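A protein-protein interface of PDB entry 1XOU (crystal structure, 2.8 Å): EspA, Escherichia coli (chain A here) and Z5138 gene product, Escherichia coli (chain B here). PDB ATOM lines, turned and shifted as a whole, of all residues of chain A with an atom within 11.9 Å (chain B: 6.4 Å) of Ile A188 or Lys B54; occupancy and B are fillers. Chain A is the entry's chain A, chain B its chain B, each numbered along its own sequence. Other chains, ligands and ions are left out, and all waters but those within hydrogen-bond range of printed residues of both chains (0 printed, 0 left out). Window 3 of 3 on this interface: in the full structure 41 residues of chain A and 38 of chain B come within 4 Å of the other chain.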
ATOM      1  N   ASP A  31      14.537  17.668 -33.816  1.00  0.00           N
ATOM      2  CA  ASP A  31      14.564  18.598 -32.647  1.00  0.00           C
ATOM      3  C   ASP A  31      15.660  18.277 -31.610  1.00  0.00           C
ATOM      4  O   ASP A  31      15.732  17.169 -31.060  1.00  0.00           O
ATOM      5  CB  ASP A  31      13.194  18.619 -31.962  1.00  0.00           C
ATOM      6  CG  ASP A  31      13.184  19.499 -30.730  1.00  0.00           C
ATOM      7  OD1 ASP A  31      13.653  20.657 -30.815  1.00  0.00           O
ATOM      8  OD2 ASP A  31      12.710  19.029 -29.682  1.00  0.00           O
ATOM      9  N   VAL A  32      16.488  19.279 -31.331  1.00  0.00           N
ATOM     10  CA  VAL A  32      17.605  19.133 -30.407  1.00  0.00           C
ATOM     11  C   VAL A  32      17.276  18.875 -28.943  1.00  0.00           C
ATOM     12  O   VAL A  32      18.046  18.205 -28.263  1.00  0.00           O
ATOM     13  CB  VAL A  32      18.539  20.366 -30.478  1.00  0.00           C
ATOM     14  CG1 VAL A  32      18.998  20.568 -31.895  1.00  0.00           C
ATOM     15  CG2 VAL A  32      17.814  21.611 -29.995  1.00  0.00           C
ATOM     16  N   ILE A  33      16.151  19.401 -28.455  1.00  0.00           N
ATOM     17  CA  ILE A  33      15.779  19.228 -27.049  1.00  0.00           C
ATOM     18  C   ILE A  33      14.580  18.315 -26.821  1.00  0.00           C
ATOM     19  O   ILE A  33      13.823  18.497 -25.863  1.00  0.00           O
ATOM     20  CB  ILE A  33      15.476  20.592 -26.365  1.00  0.00           C
ATOM     21  CG1 ILE A  33      14.314  21.283 -27.074  1.00  0.00           C
ATOM     22  CG2 ILE A  33      16.710  21.498 -26.394  1.00  0.00           C
ATOM     23  CD1 ILE A  33      13.839  22.540 -26.374  1.00  0.00           C
ATOM     24  N   ASP A  34      14.413  17.337 -27.708  1.00  0.00           N
ATOM     25  CA  ASP A  34      13.324  16.361 -27.626  1.00  0.00           C
ATOM     26  C   ASP A  34      11.959  16.942 -27.239  1.00  0.00           C
ATOM     27  O   ASP A  34      11.256  16.431 -26.370  1.00  0.00           O
ATOM     28  CB  ASP A  34      13.714  15.227 -26.667  1.00  0.00           C
ATOM     29  CG  ASP A  34      12.660  14.119 -26.607  1.00  0.00           C
ATOM     30  OD1 ASP A  34      12.180  13.695 -27.699  1.00  0.00           O
ATOM     31  OD2 ASP A  34      12.323  13.681 -25.466  1.00  0.00           O
ATOM     32  N   LEU A  35      11.589  18.018 -27.909  1.00  0.00           N
ATOM     33  CA  LEU A  35      10.319  18.677 -27.687  1.00  0.00           C
ATOM     34  C   LEU A  35       9.188  17.773 -28.199  1.00  0.00           C
ATOM     35  O   LEU A  35       8.095  17.734 -27.638  1.00  0.00           O
ATOM     36  CB  LEU A  35      10.331  20.009 -28.428  1.00  0.00           C
ATOM     37  CG  LEU A  35      10.012  21.256 -27.614  1.00  0.00           C
ATOM     38  CD1 LEU A  35      10.396  21.061 -26.144  1.00  0.00           C
ATOM     39  CD2 LEU A  35      10.746  22.440 -28.250  1.00  0.00           C
ATOM     40  N   LEU A  39       6.096  17.489 -25.674  1.00  0.00           N
ATOM     41  CA  LEU A  39       4.832  18.053 -26.116  1.00  0.00           C
ATOM     42  C   LEU A  39       3.794  17.012 -26.520  1.00  0.00           C
ATOM     43  O   LEU A  39       2.592  17.223 -26.331  1.00  0.00           O
ATOM     44  CB  LEU A  39       5.072  19.017 -27.279  1.00  0.00           C
ATOM     45  CG  LEU A  39       5.583  20.418 -26.920  1.00  0.00           C
ATOM     46  CD1 LEU A  39       4.497  21.199 -26.179  1.00  0.00           C
ATOM     47  CD2 LEU A  39       6.823  20.299 -26.046  1.00  0.00           C
ATOM     48  N   GLN A 178       3.466  28.322 -19.552  1.00  0.00           N
ATOM     49  CA  GLN A 178       3.827  29.662 -20.000  1.00  0.00           C
ATOM     50  C   GLN A 178       5.234  30.040 -19.560  1.00  0.00           C
ATOM     51  O   GLN A 178       6.020  30.572 -20.350  1.00  0.00           O
ATOM     52  CB  GLN A 178       2.812  30.664 -19.477  1.00  0.00           C
ATOM     53  CG  GLN A 178       1.697  30.919 -20.461  1.00  0.00           C
ATOM     54  CD  GLN A 178       0.552  31.681 -19.850  1.00  0.00           C
ATOM     55  OE1 GLN A 178      -0.205  32.327 -20.557  1.00  0.00           O
ATOM     56  NE2 GLN A 178       0.408  31.599 -18.529  1.00  0.00           N
ATOM     57  N   SER A 179       5.542  29.756 -18.297  1.00  0.00           N
ATOM     58  CA  SER A 179       6.863  30.022 -17.747  1.00  0.00           C
ATOM     59  C   SER A 179       7.853  29.229 -18.589  1.00  0.00           C
ATOM     60  O   SER A 179       8.940  29.708 -18.911  1.00  0.00           O
ATOM     61  CB  SER A 179       6.938  29.545 -16.300  1.00  0.00           C
ATOM     62  OG  SER A 179       5.908  30.118 -15.528  1.00  0.00           O
ATOM     63  N   LEU A 180       7.461  28.007 -18.944  1.00  0.00           N
ATOM     64  CA  LEU A 180       8.304  27.148 -19.756  1.00  0.00           C
ATOM     65  C   LEU A 180       8.650  27.911 -21.017  1.00  0.00           C
ATOM     66  O   LEU A 180       9.823  28.105 -21.325  1.00  0.00           O
ATOM     67  CB  LEU A 180       7.567  25.865 -20.129  1.00  0.00           C
ATOM     68  CG  LEU A 180       8.379  24.568 -20.220  1.00  0.00           C
ATOM     69  CD1 LEU A 180       7.644  23.657 -21.191  1.00  0.00           C
ATOM     70  CD2 LEU A 180       9.809  24.812 -20.684  1.00  0.00           C
ATOM     71  N   GLN A 181       7.617  28.342 -21.735  1.00  0.00           N
ATOM     72  CA  GLN A 181       7.797  29.098 -22.964  1.00  0.00           C
ATOM     73  C   GLN A 181       8.678  30.320 -22.756  1.00  0.00           C
ATOM     74  O   GLN A 181       9.619  30.560 -23.519  1.00  0.00           O
ATOM     75  CB  GLN A 181       6.450  29.571 -23.504  1.00  0.00           C
ATOM     76  CG  GLN A 181       5.932  28.801 -24.704  1.00  0.00           C
ATOM     77  CD  GLN A 181       4.761  29.501 -25.378  1.00  0.00           C
ATOM     78  OE1 GLN A 181       4.120  28.944 -26.275  1.00  0.00           O
ATOM     79  NE2 GLN A 181       4.481  30.730 -24.953  1.00  0.00           N
ATOM     80  N   TYR A 182       8.358  31.102 -21.732  1.00  0.00           N
ATOM     81  CA  TYR A 182       9.108  32.314 -21.440  1.00  0.00           C
ATOM     82  C   TYR A 182      10.587  32.016 -21.165  1.00  0.00           C
ATOM     83  O   TYR A 182      11.472  32.611 -21.788  1.00  0.00           O
ATOM     84  CB  TYR A 182       8.462  33.048 -20.257  1.00  0.00           C
ATOM     85  CG  TYR A 182       9.183  34.311 -19.825  1.00  0.00           C
ATOM     86  CD1 TYR A 182      10.077  34.296 -18.744  1.00  0.00           C
ATOM     87  CD2 TYR A 182       8.977  35.523 -20.496  1.00  0.00           C
ATOM     88  CE1 TYR A 182      10.746  35.456 -18.340  1.00  0.00           C
ATOM     89  CE2 TYR A 182       9.644  36.691 -20.100  1.00  0.00           C
ATOM     90  CZ  TYR A 182      10.524  36.647 -19.024  1.00  0.00           C
ATOM     91  OH  TYR A 182      11.185  37.792 -18.631  1.00  0.00           O
ATOM     92  N   ARG A 183      10.854  31.094 -20.241  1.00  0.00           N
ATOM     93  CA  ARG A 183      12.226  30.737 -19.918  1.00  0.00           C
ATOM     94  C   ARG A 183      12.961  30.178 -21.140  1.00  0.00           C
ATOM     95  O   ARG A 183      14.134  30.490 -21.355  1.00  0.00           O
ATOM     96  CB  ARG A 183      12.269  29.729 -18.761  1.00  0.00           C
ATOM     97  CG  ARG A 183      11.898  30.344 -17.415  1.00  0.00           C
ATOM     98  CD  ARG A 183      12.263  29.452 -16.221  1.00  0.00           C
ATOM     99  NE  ARG A 183      13.664  29.025 -16.266  1.00  0.00           N
ATOM    100  CZ  ARG A 183      14.437  28.814 -15.198  1.00  0.00           C
ATOM    101  NH1 ARG A 183      15.697  28.421 -15.349  1.00  0.00           N
ATOM    102  NH2 ARG A 183      13.958  29.016 -13.979  1.00  0.00           N
ATOM    103  N   THR A 184      12.281  29.367 -21.948  1.00  0.00           N
ATOM    104  CA  THR A 184      12.926  28.807 -23.133  1.00  0.00           C
ATOM    105  C   THR A 184      13.351  29.939 -24.051  1.00  0.00           C
ATOM    106  O   THR A 184      14.528  30.092 -24.359  1.00  0.00           O
ATOM    107  CB  THR A 184      11.980  27.878 -23.925  1.00  0.00           C
ATOM    108  OG1 THR A 184      11.571  26.792 -23.092  1.00  0.00           O
ATOM    109  CG2 THR A 184      12.680  27.319 -25.150  1.00  0.00           C
ATOM    110  N   ILE A 185      12.378  30.735 -24.475  1.00  0.00           N
ATOM    111  CA  ILE A 185      12.616  31.854 -25.370  1.00  0.00           C
ATOM    112  C   ILE A 185      13.632  32.829 -24.811  1.00  0.00           C
ATOM    113  O   ILE A 185      14.470  33.358 -25.540  1.00  0.00           O
ATOM    114  CB  ILE A 185      11.293  32.565 -25.681  1.00  0.00           C
ATOM    115  CG1 ILE A 185      10.519  31.720 -26.694  1.00  0.00           C
ATOM    116  CG2 ILE A 185      11.542  33.989 -26.178  1.00  0.00           C
ATOM    117  CD1 ILE A 185       9.174  32.261 -27.026  1.00  0.00           C
ATOM    118  N   SER A 186      13.557  33.074 -23.512  1.00  0.00           N
ATOM    119  CA  SER A 186      14.514  33.962 -22.878  1.00  0.00           C
ATOM    120  C   SER A 186      15.909  33.358 -23.066  1.00  0.00           C
ATOM    121  O   SER A 186      16.847  34.044 -23.458  1.00  0.00           O
ATOM    122  CB  SER A 186      14.195  34.096 -21.391  1.00  0.00           C
ATOM    123  OG  SER A 186      15.351  34.483 -20.672  1.00  0.00           O
ATOM    124  N   GLY A 187      16.024  32.059 -22.798  1.00  0.00           N
ATOM    125  CA  GLY A 187      17.293  31.366 -22.933  1.00  0.00           C
ATOM    126  C   GLY A 187      17.854  31.313 -24.345  1.00  0.00           C
ATOM    127  O   GLY A 187      19.068  31.331 -24.531  1.00  0.00           O
ATOM    128  N   ILE A 188      16.985  31.240 -25.347  1.00  0.00           N
ATOM    129  CA  ILE A 188      17.440  31.196 -26.731  1.00  0.00           C
ATOM    130  C   ILE A 188      17.945  32.565 -27.171  1.00  0.00           C
ATOM    131  O   ILE A 188      18.598  32.689 -28.205  1.00  0.00           O
ATOM    132  CB  ILE A 188      16.309  30.777 -27.695  1.00  0.00           C
ATOM    133  CG1 ILE A 188      15.791  29.387 -27.329  1.00  0.00           C
ATOM    134  CG2 ILE A 188      16.820  30.760 -29.119  1.00  0.00           C
ATOM    135  CD1 ILE A 188      14.709  28.857 -28.261  1.00  0.00           C
ATOM    136  N   SER A 189      17.656  33.594 -26.383  1.00  0.00           N
ATOM    137  CA  SER A 189      18.079  34.940 -26.744  1.00  0.00           C
ATOM    138  C   SER A 189      19.077  35.580 -25.782  1.00  0.00           C
ATOM    139  O   SER A 189      19.392  36.762 -25.924  1.00  0.00           O
ATOM    140  CB  SER A 189      16.853  35.849 -26.885  1.00  0.00           C
ATOM    141  OG  SER A 189      16.199  36.022 -25.641  1.00  0.00           O
ATOM    142  N   LEU A 190      19.570  34.810 -24.811  1.00  0.00           N
ATOM    143  CA  LEU A 190      20.544  35.304 -23.828  1.00  0.00           C
ATOM    144  C   LEU A 190      20.728  34.359 -22.639  1.00  0.00           C
ATOM    145  O   LEU A 190      20.195  33.231 -22.684  1.00  0.00           O
ATOM    146  CB  LEU A 190      20.137  36.683 -23.298  1.00  0.00           C
ATOM    147  CG  LEU A 190      18.761  36.799 -22.636  1.00  0.00           C
ATOM    148  CD1 LEU A 190      18.916  37.396 -21.244  1.00  0.00           C
ATOM    149  CD2 LEU A 190      17.844  37.657 -23.502  1.00  0.00           C
ATOM    150  N   VAL B  33       6.985  27.191 -32.747  1.00  0.00           N
ATOM    151  CA  VAL B  33       7.827  28.356 -32.983  1.00  0.00           C
ATOM    152  C   VAL B  33       9.060  28.142 -32.112  1.00  0.00           C
ATOM    153  O   VAL B  33      10.186  28.422 -32.516  1.00  0.00           O
ATOM    154  CB  VAL B  33       7.124  29.663 -32.551  1.00  0.00           C
ATOM    155  CG1 VAL B  33       8.056  30.851 -32.735  1.00  0.00           C
ATOM    156  CG2 VAL B  33       5.874  29.857 -33.367  1.00  0.00           C
ATOM    157  N   VAL B  34       8.835  27.634 -30.908  1.00  0.00           N
ATOM    158  CA  VAL B  34       9.933  27.360 -30.002  1.00  0.00           C
ATOM    159  C   VAL B  34      10.803  26.270 -30.622  1.00  0.00           C
ATOM    160  O   VAL B  34      12.019  26.307 -30.516  1.00  0.00           O
ATOM    161  CB  VAL B  34       9.424  26.897 -28.635  1.00  0.00           C
ATOM    162  CG1 VAL B  34      10.588  26.448 -27.784  1.00  0.00           C
ATOM    163  CG2 VAL B  34       8.684  28.037 -27.941  1.00  0.00           C
ATOM    164  N   SER B  37      12.843  27.865 -33.466  1.00  0.00           N
ATOM    165  CA  SER B  37      13.851  28.743 -32.888  1.00  0.00           C
ATOM    166  C   SER B  37      15.040  27.954 -32.388  1.00  0.00           C
ATOM    167  O   SER B  37      16.191  28.308 -32.649  1.00  0.00           O
ATOM    168  CB  SER B  37      13.268  29.530 -31.716  1.00  0.00           C
ATOM    169  OG  SER B  37      11.981  30.030 -32.023  1.00  0.00           O
ATOM    170  N   VAL B  38      14.747  26.882 -31.659  1.00  0.00           N
ATOM    171  CA  VAL B  38      15.772  26.022 -31.073  1.00  0.00           C
ATOM    172  C   VAL B  38      16.644  25.359 -32.141  1.00  0.00           C
ATOM    173  O   VAL B  38      17.838  25.160 -31.930  1.00  0.00           O
ATOM    174  CB  VAL B  38      15.125  24.948 -30.152  1.00  0.00           C
ATOM    175  CG1 VAL B  38      14.917  23.635 -30.911  1.00  0.00           C
ATOM    176  CG2 VAL B  38      15.971  24.765 -28.909  1.00  0.00           C
ATOM    177  N   LEU B  41      18.974  27.950 -33.395  1.00  0.00           N
ATOM    178  CA  LEU B  41      20.074  28.132 -32.456  1.00  0.00           C
ATOM    179  C   LEU B  41      21.160  27.091 -32.730  1.00  0.00           C
ATOM    180  O   LEU B  41      22.334  27.342 -32.496  1.00  0.00           O
ATOM    181  CB  LEU B  41      19.597  27.990 -31.014  1.00  0.00           C
ATOM    182  CG  LEU B  41      20.205  29.010 -30.044  1.00  0.00           C
ATOM    183  CD1 LEU B  41      20.114  28.481 -28.619  1.00  0.00           C
ATOM    184  CD2 LEU B  41      21.645  29.280 -30.415  1.00  0.00           C
ATOM    185  N   LYS B  44      23.270  28.155 -35.788  1.00  0.00           N
ATOM    186  CA  LYS B  44      24.178  29.221 -35.389  1.00  0.00           C
ATOM    187  C   LYS B  44      25.287  28.692 -34.484  1.00  0.00           C
ATOM    188  O   LYS B  44      26.380  29.251 -34.443  1.00  0.00           O
ATOM    189  CB  LYS B  44      23.416  30.361 -34.689  1.00  0.00           C
ATOM    190  CG  LYS B  44      24.227  31.673 -34.598  1.00  0.00           C
ATOM    191  CD  LYS B  44      23.419  32.871 -34.068  1.00  0.00           C
ATOM    192  CE  LYS B  44      23.232  32.830 -32.545  1.00  0.00           C
ATOM    193  NZ  LYS B  44      22.456  33.985 -31.973  1.00  0.00           N
ATOM    194  N   ASP B  48      29.196  29.646 -34.206  1.00  0.00           N
ATOM    195  CA  ASP B  48      29.268  30.491 -33.020  1.00  0.00           C
ATOM    196  C   ASP B  48      29.197  29.735 -31.690  1.00  0.00           C
ATOM    197  O   ASP B  48      28.243  29.002 -31.430  1.00  0.00           O
ATOM    198  CB  ASP B  48      28.151  31.533 -33.095  1.00  0.00           C
ATOM    199  CG  ASP B  48      28.148  32.469 -31.915  1.00  0.00           C
ATOM    200  OD1 ASP B  48      27.428  33.488 -31.978  1.00  0.00           O
ATOM    201  OD2 ASP B  48      28.857  32.188 -30.923  1.00  0.00           O
ATOM    202  N   PRO B  49      30.212  29.919 -30.824  1.00  0.00           N
ATOM    203  CA  PRO B  49      30.290  29.267 -29.513  1.00  0.00           C
ATOM    204  C   PRO B  49      29.402  29.907 -28.450  1.00  0.00           C
ATOM    205  O   PRO B  49      29.193  29.333 -27.382  1.00  0.00           O
ATOM    206  CB  PRO B  49      31.771  29.371 -29.171  1.00  0.00           C
ATOM    207  CG  PRO B  49      32.134  30.683 -29.750  1.00  0.00           C
ATOM    208  CD  PRO B  49      31.464  30.641 -31.110  1.00  0.00           C
ATOM    209  N   GLN B  50      28.894  31.102 -28.733  1.00  0.00           N
ATOM    210  CA  GLN B  50      28.011  31.785 -27.796  1.00  0.00           C
ATOM    211  C   GLN B  50      26.693  31.025 -27.893  1.00  0.00           C
ATOM    212  O   GLN B  50      26.017  30.781 -26.899  1.00  0.00           O
ATOM    213  CB  GLN B  50      27.800  33.245 -28.221  1.00  0.00           C
ATOM    214  CG  GLN B  50      27.576  34.229 -27.066  1.00  0.00           C
ATOM    215  CD  GLN B  50      28.872  34.608 -26.338  1.00  0.00           C
ATOM    216  OE1 GLN B  50      29.795  35.177 -26.939  1.00  0.00           O
ATOM    217  NE2 GLN B  50      28.942  34.293 -25.039  1.00  0.00           N
ATOM    218  N   ALA B  51      26.349  30.646 -29.118  1.00  0.00           N
ATOM    219  CA  ALA B  51      25.131  29.900 -29.388  1.00  0.00           C
ATOM    220  C   ALA B  51      25.246  28.497 -28.794  1.00  0.00           C
ATOM    221  O   ALA B  51      24.309  27.985 -28.188  1.00  0.00           O
ATOM    222  CB  ALA B  51      24.899  29.818 -30.905  1.00  0.00           C
ATOM    223  N   ALA B  52      26.408  27.883 -28.976  1.00  0.00           N
ATOM    224  CA  ALA B  52      26.651  26.542 -28.470  1.00  0.00           C
ATOM    225  C   ALA B  52      26.450  26.486 -26.960  1.00  0.00           C
ATOM    226  O   ALA B  52      25.841  25.552 -26.444  1.00  0.00           O
ATOM    227  CB  ALA B  52      28.062  26.102 -28.835  1.00  0.00           C
ATOM    228  N   GLU B  53      26.964  27.488 -26.254  1.00  0.00           N
ATOM    229  CA  GLU B  53      26.835  27.545 -24.807  1.00  0.00           C
ATOM    230  C   GLU B  53      25.368  27.730 -24.397  1.00  0.00           C
ATOM    231  O   GLU B  53      24.930  27.203 -23.372  1.00  0.00           O
ATOM    232  CB  GLU B  53      27.684  28.686 -24.260  1.00  0.00           C
ATOM    233  CG  GLU B  53      27.677  28.798 -22.745  1.00  0.00           C
ATOM    234  CD  GLU B  53      28.316  27.593 -22.055  1.00  0.00           C
ATOM    235  OE1 GLU B  53      28.327  27.565 -20.796  1.00  0.00           O
ATOM    236  OE2 GLU B  53      28.803  26.682 -22.772  1.00  0.00           O
ATOM    237  N   LYS B  54      24.616  28.487 -25.195  1.00  0.00           N
ATOM    238  CA  LYS B  54      23.201  28.714 -24.930  1.00  0.00           C
ATOM    239  C   LYS B  54      22.472  27.390 -25.088  1.00  0.00           C
ATOM    240  O   LYS B  54      21.762  26.945 -24.189  1.00  0.00           O
ATOM    241  CB  LYS B  54      22.619  29.752 -25.908  1.00  0.00           C
ATOM    242  CG  LYS B  54      22.899  31.211 -25.518  1.00  0.00           C
ATOM    243  CD  LYS B  54      22.230  32.233 -26.460  1.00  0.00           C
ATOM    244  CE  LYS B  54      22.845  32.203 -27.868  1.00  0.00           C
ATOM    245  NZ  LYS B  54      22.281  33.210 -28.844  1.00  0.00           N
ATOM    246  N   LEU B  55      22.661  26.759 -26.237  1.00  0.00           N
ATOM    247  CA  LEU B  55      22.029  25.482 -26.523  1.00  0.00           C
ATOM    248  C   LEU B  55      22.255  24.463 -25.408  1.00  0.00           C
ATOM    249  O   LEU B  55      21.298  23.879 -24.898  1.00  0.00           O
ATOM    250  CB  LEU B  55      22.563  24.911 -27.838  1.00  0.00           C
ATOM    251  CG  LEU B  55      21.521  24.389 -28.833  1.00  0.00           C
ATOM    252  CD1 LEU B  55      22.223  23.631 -29.956  1.00  0.00           C
ATOM    253  CD2 LEU B  55      20.524  23.490 -28.117  1.00  0.00           C
ATOM    254  N   ASN B  56      23.514  24.253 -25.026  1.00  0.00           N
ATOM    255  CA  ASN B  56      23.840  23.287 -23.979  1.00  0.00           C
ATOM    256  C   ASN B  56      23.163  23.615 -22.659  1.00  0.00           C
ATOM    257  O   ASN B  56      22.752  22.719 -21.920  1.00  0.00           O
ATOM    258  CB  ASN B  56      25.349  23.198 -23.767  1.00  0.00           C
ATOM    259  CG  ASN B  56      26.103  22.883 -25.041  1.00  0.00           C
ATOM    260  OD1 ASN B  56      25.631  22.131 -25.892  1.00  0.00           O
ATOM    261  ND2 ASN B  56      27.295  23.452 -25.171  1.00  0.00           N
ATOM    262  N   LYS B  57      23.067  24.903 -22.353  1.00  0.00           N
ATOM    263  CA  LYS B  57      22.403  25.336 -21.128  1.00  0.00           C
ATOM    264  C   LYS B  57      20.928  24.946 -21.241  1.00  0.00           C
ATOM    265  O   LYS B  57      20.329  24.459 -20.281  1.00  0.00           O
ATOM    266  CB  LYS B  57      22.551  26.859 -20.932  1.00  0.00           C
ATOM    267  CG  LYS B  57      23.852  27.254 -20.242  1.00  0.00           C
ATOM    268  CD  LYS B  57      23.980  26.448 -18.947  1.00  0.00           C
ATOM    269  CE  LYS B  57      25.416  26.375 -18.420  1.00  0.00           C
ATOM    270  NZ  LYS B  57      25.560  25.281 -17.388  1.00  0.00           N
ATOM    271  N   LEU B  58      20.361  25.155 -22.428  1.00  0.00           N
ATOM    272  CA  LEU B  58      18.967  24.811 -22.696  1.00  0.00           C
ATOM    273  C   LEU B  58      18.758  23.315 -22.550  1.00  0.00           C
ATOM    274  O   LEU B  58      17.831  22.861 -21.873  1.00  0.00           O
ATOM    275  CB  LEU B  58      18.582  25.218 -24.112  1.00  0.00           C
ATOM    276  CG  LEU B  58      17.681  26.446 -24.232  1.00  0.00           C
ATOM    277  CD1 LEU B  58      17.405  26.717 -25.701  1.00  0.00           C
ATOM    278  CD2 LEU B  58      16.387  26.208 -23.480  1.00  0.00           C
ATOM    279  N   ILE B  59      19.623  22.548 -23.201  1.00  0.00           N
ATOM    280  CA  ILE B  59      19.544  21.096 -23.140  1.00  0.00           C
ATOM    281  C   ILE B  59      19.571  20.601 -21.692  1.00  0.00           C
ATOM    282  O   ILE B  59      18.737  19.795 -21.298  1.00  0.00           O
ATOM    283  CB  ILE B  59      20.693  20.462 -23.943  1.00  0.00           C
ATOM    284  CG1 ILE B  59      20.563  20.877 -25.411  1.00  0.00           C
ATOM    285  CG2 ILE B  59      20.664  18.946 -23.797  1.00  0.00           C
ATOM    286  CD1 ILE B  59      21.765  20.561 -26.262  1.00  0.00           C
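The backbone carbonyl oxygen (O) of Leu A180 sits at hydrogen-bond distance from the side-chain hydroxyl (OG1) of Thr A184 (2.8 Å).
The side-chain hydroxyl of Ser B37 lies within hydrogen-bond range of the backbone carbonyl oxygen of Val B33 (2.5 Å).
OD2 of Asp A31 lies within hydrogen-bond range of N of Asp A34.
Val B38 touches Asp A31 (CG1 to OD1, 3.2 Å).
Val A32 touches Val B38 (CG2 to CG1, 3.7 Å).
Leu B55 touches Val A32 (CD2 to CG2, 3.8 Å).
Ile A33 touches Val B38.
Thr A184 touches Val B34.
Gly A187 touches Lys B54 (O to CD, 3.8 Å).
Ile A188 touches Ser B37.
Val B38 touches Ile A188.
Ile A188 touches Leu B41 (CG2 to CG, 3.9 Å).
Leu B58 touches Ile A188.
Ile A188 touches just these residues of chain B: Ser B37, Val B38, Leu B41, Lys B54 and Leu B58.
Of the printed residues of chain A, Lys B54 touches Gly A187 (3.8 Å) and Ile A188 (3.8 Å).
Of chain A, only Ile A188 comes within 4 Å of Ser B37.
Leu B41 touches just one residue of chain A: Ile A188 (3.9 Å).
Ala B51 touches none of the printed residues of chain A.
No residue of chain A comes within 4 Å of Ala B52.
Of chain A, only Val A32 (3.8 Å) comes within 4 Å of Leu B55.
Asn B56 touches none of the printed residues of chain A.
Printed residues of chain A within 4 Å of Leu B58: Ile A188.
Of the printed residues of chain A, Val B38 touches Asp A31, Val A32, Ile A33 and Ile A188.
Of the printed residues of chain B, Ile A33 touches Val B38.
Lys B57 touches none of the printed residues of chain A.
The nearest residue of chain B that does not touch Ile A188 is Val B34 (4.3 Å).
The nearest residue of chain A that does not touch Lys B54 is Leu A190 (4.1 Å).
The nearest printed residue of chain B that does not touch Ile A33 is Ile B59 (4.02 Å).
Of the 18 printed residues of chain B, 7 touch a printed residue of chain A.
Printed residues of chain B that touch a printed residue of chain A: Val B34, Ser B37, Val B38, Leu B41, Lys B54, Leu B55 and Leu B58.
Along chain B the printed residues that touch a printed residue of chain A span positions 34 to 58.
Of the 19 printed residues of chain A, 6 touch a printed residue of chain B.
Printed residues of chain A that touch a printed residue of chain B: Asp A31, Val A32, Ile A33, Thr A184, Gly A187 and Ile A188.
Among the printed residues, no Asp or Glu carboxylate lies within 4 Å of a Lys or Arg side-chain nitrogen of the other chain.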
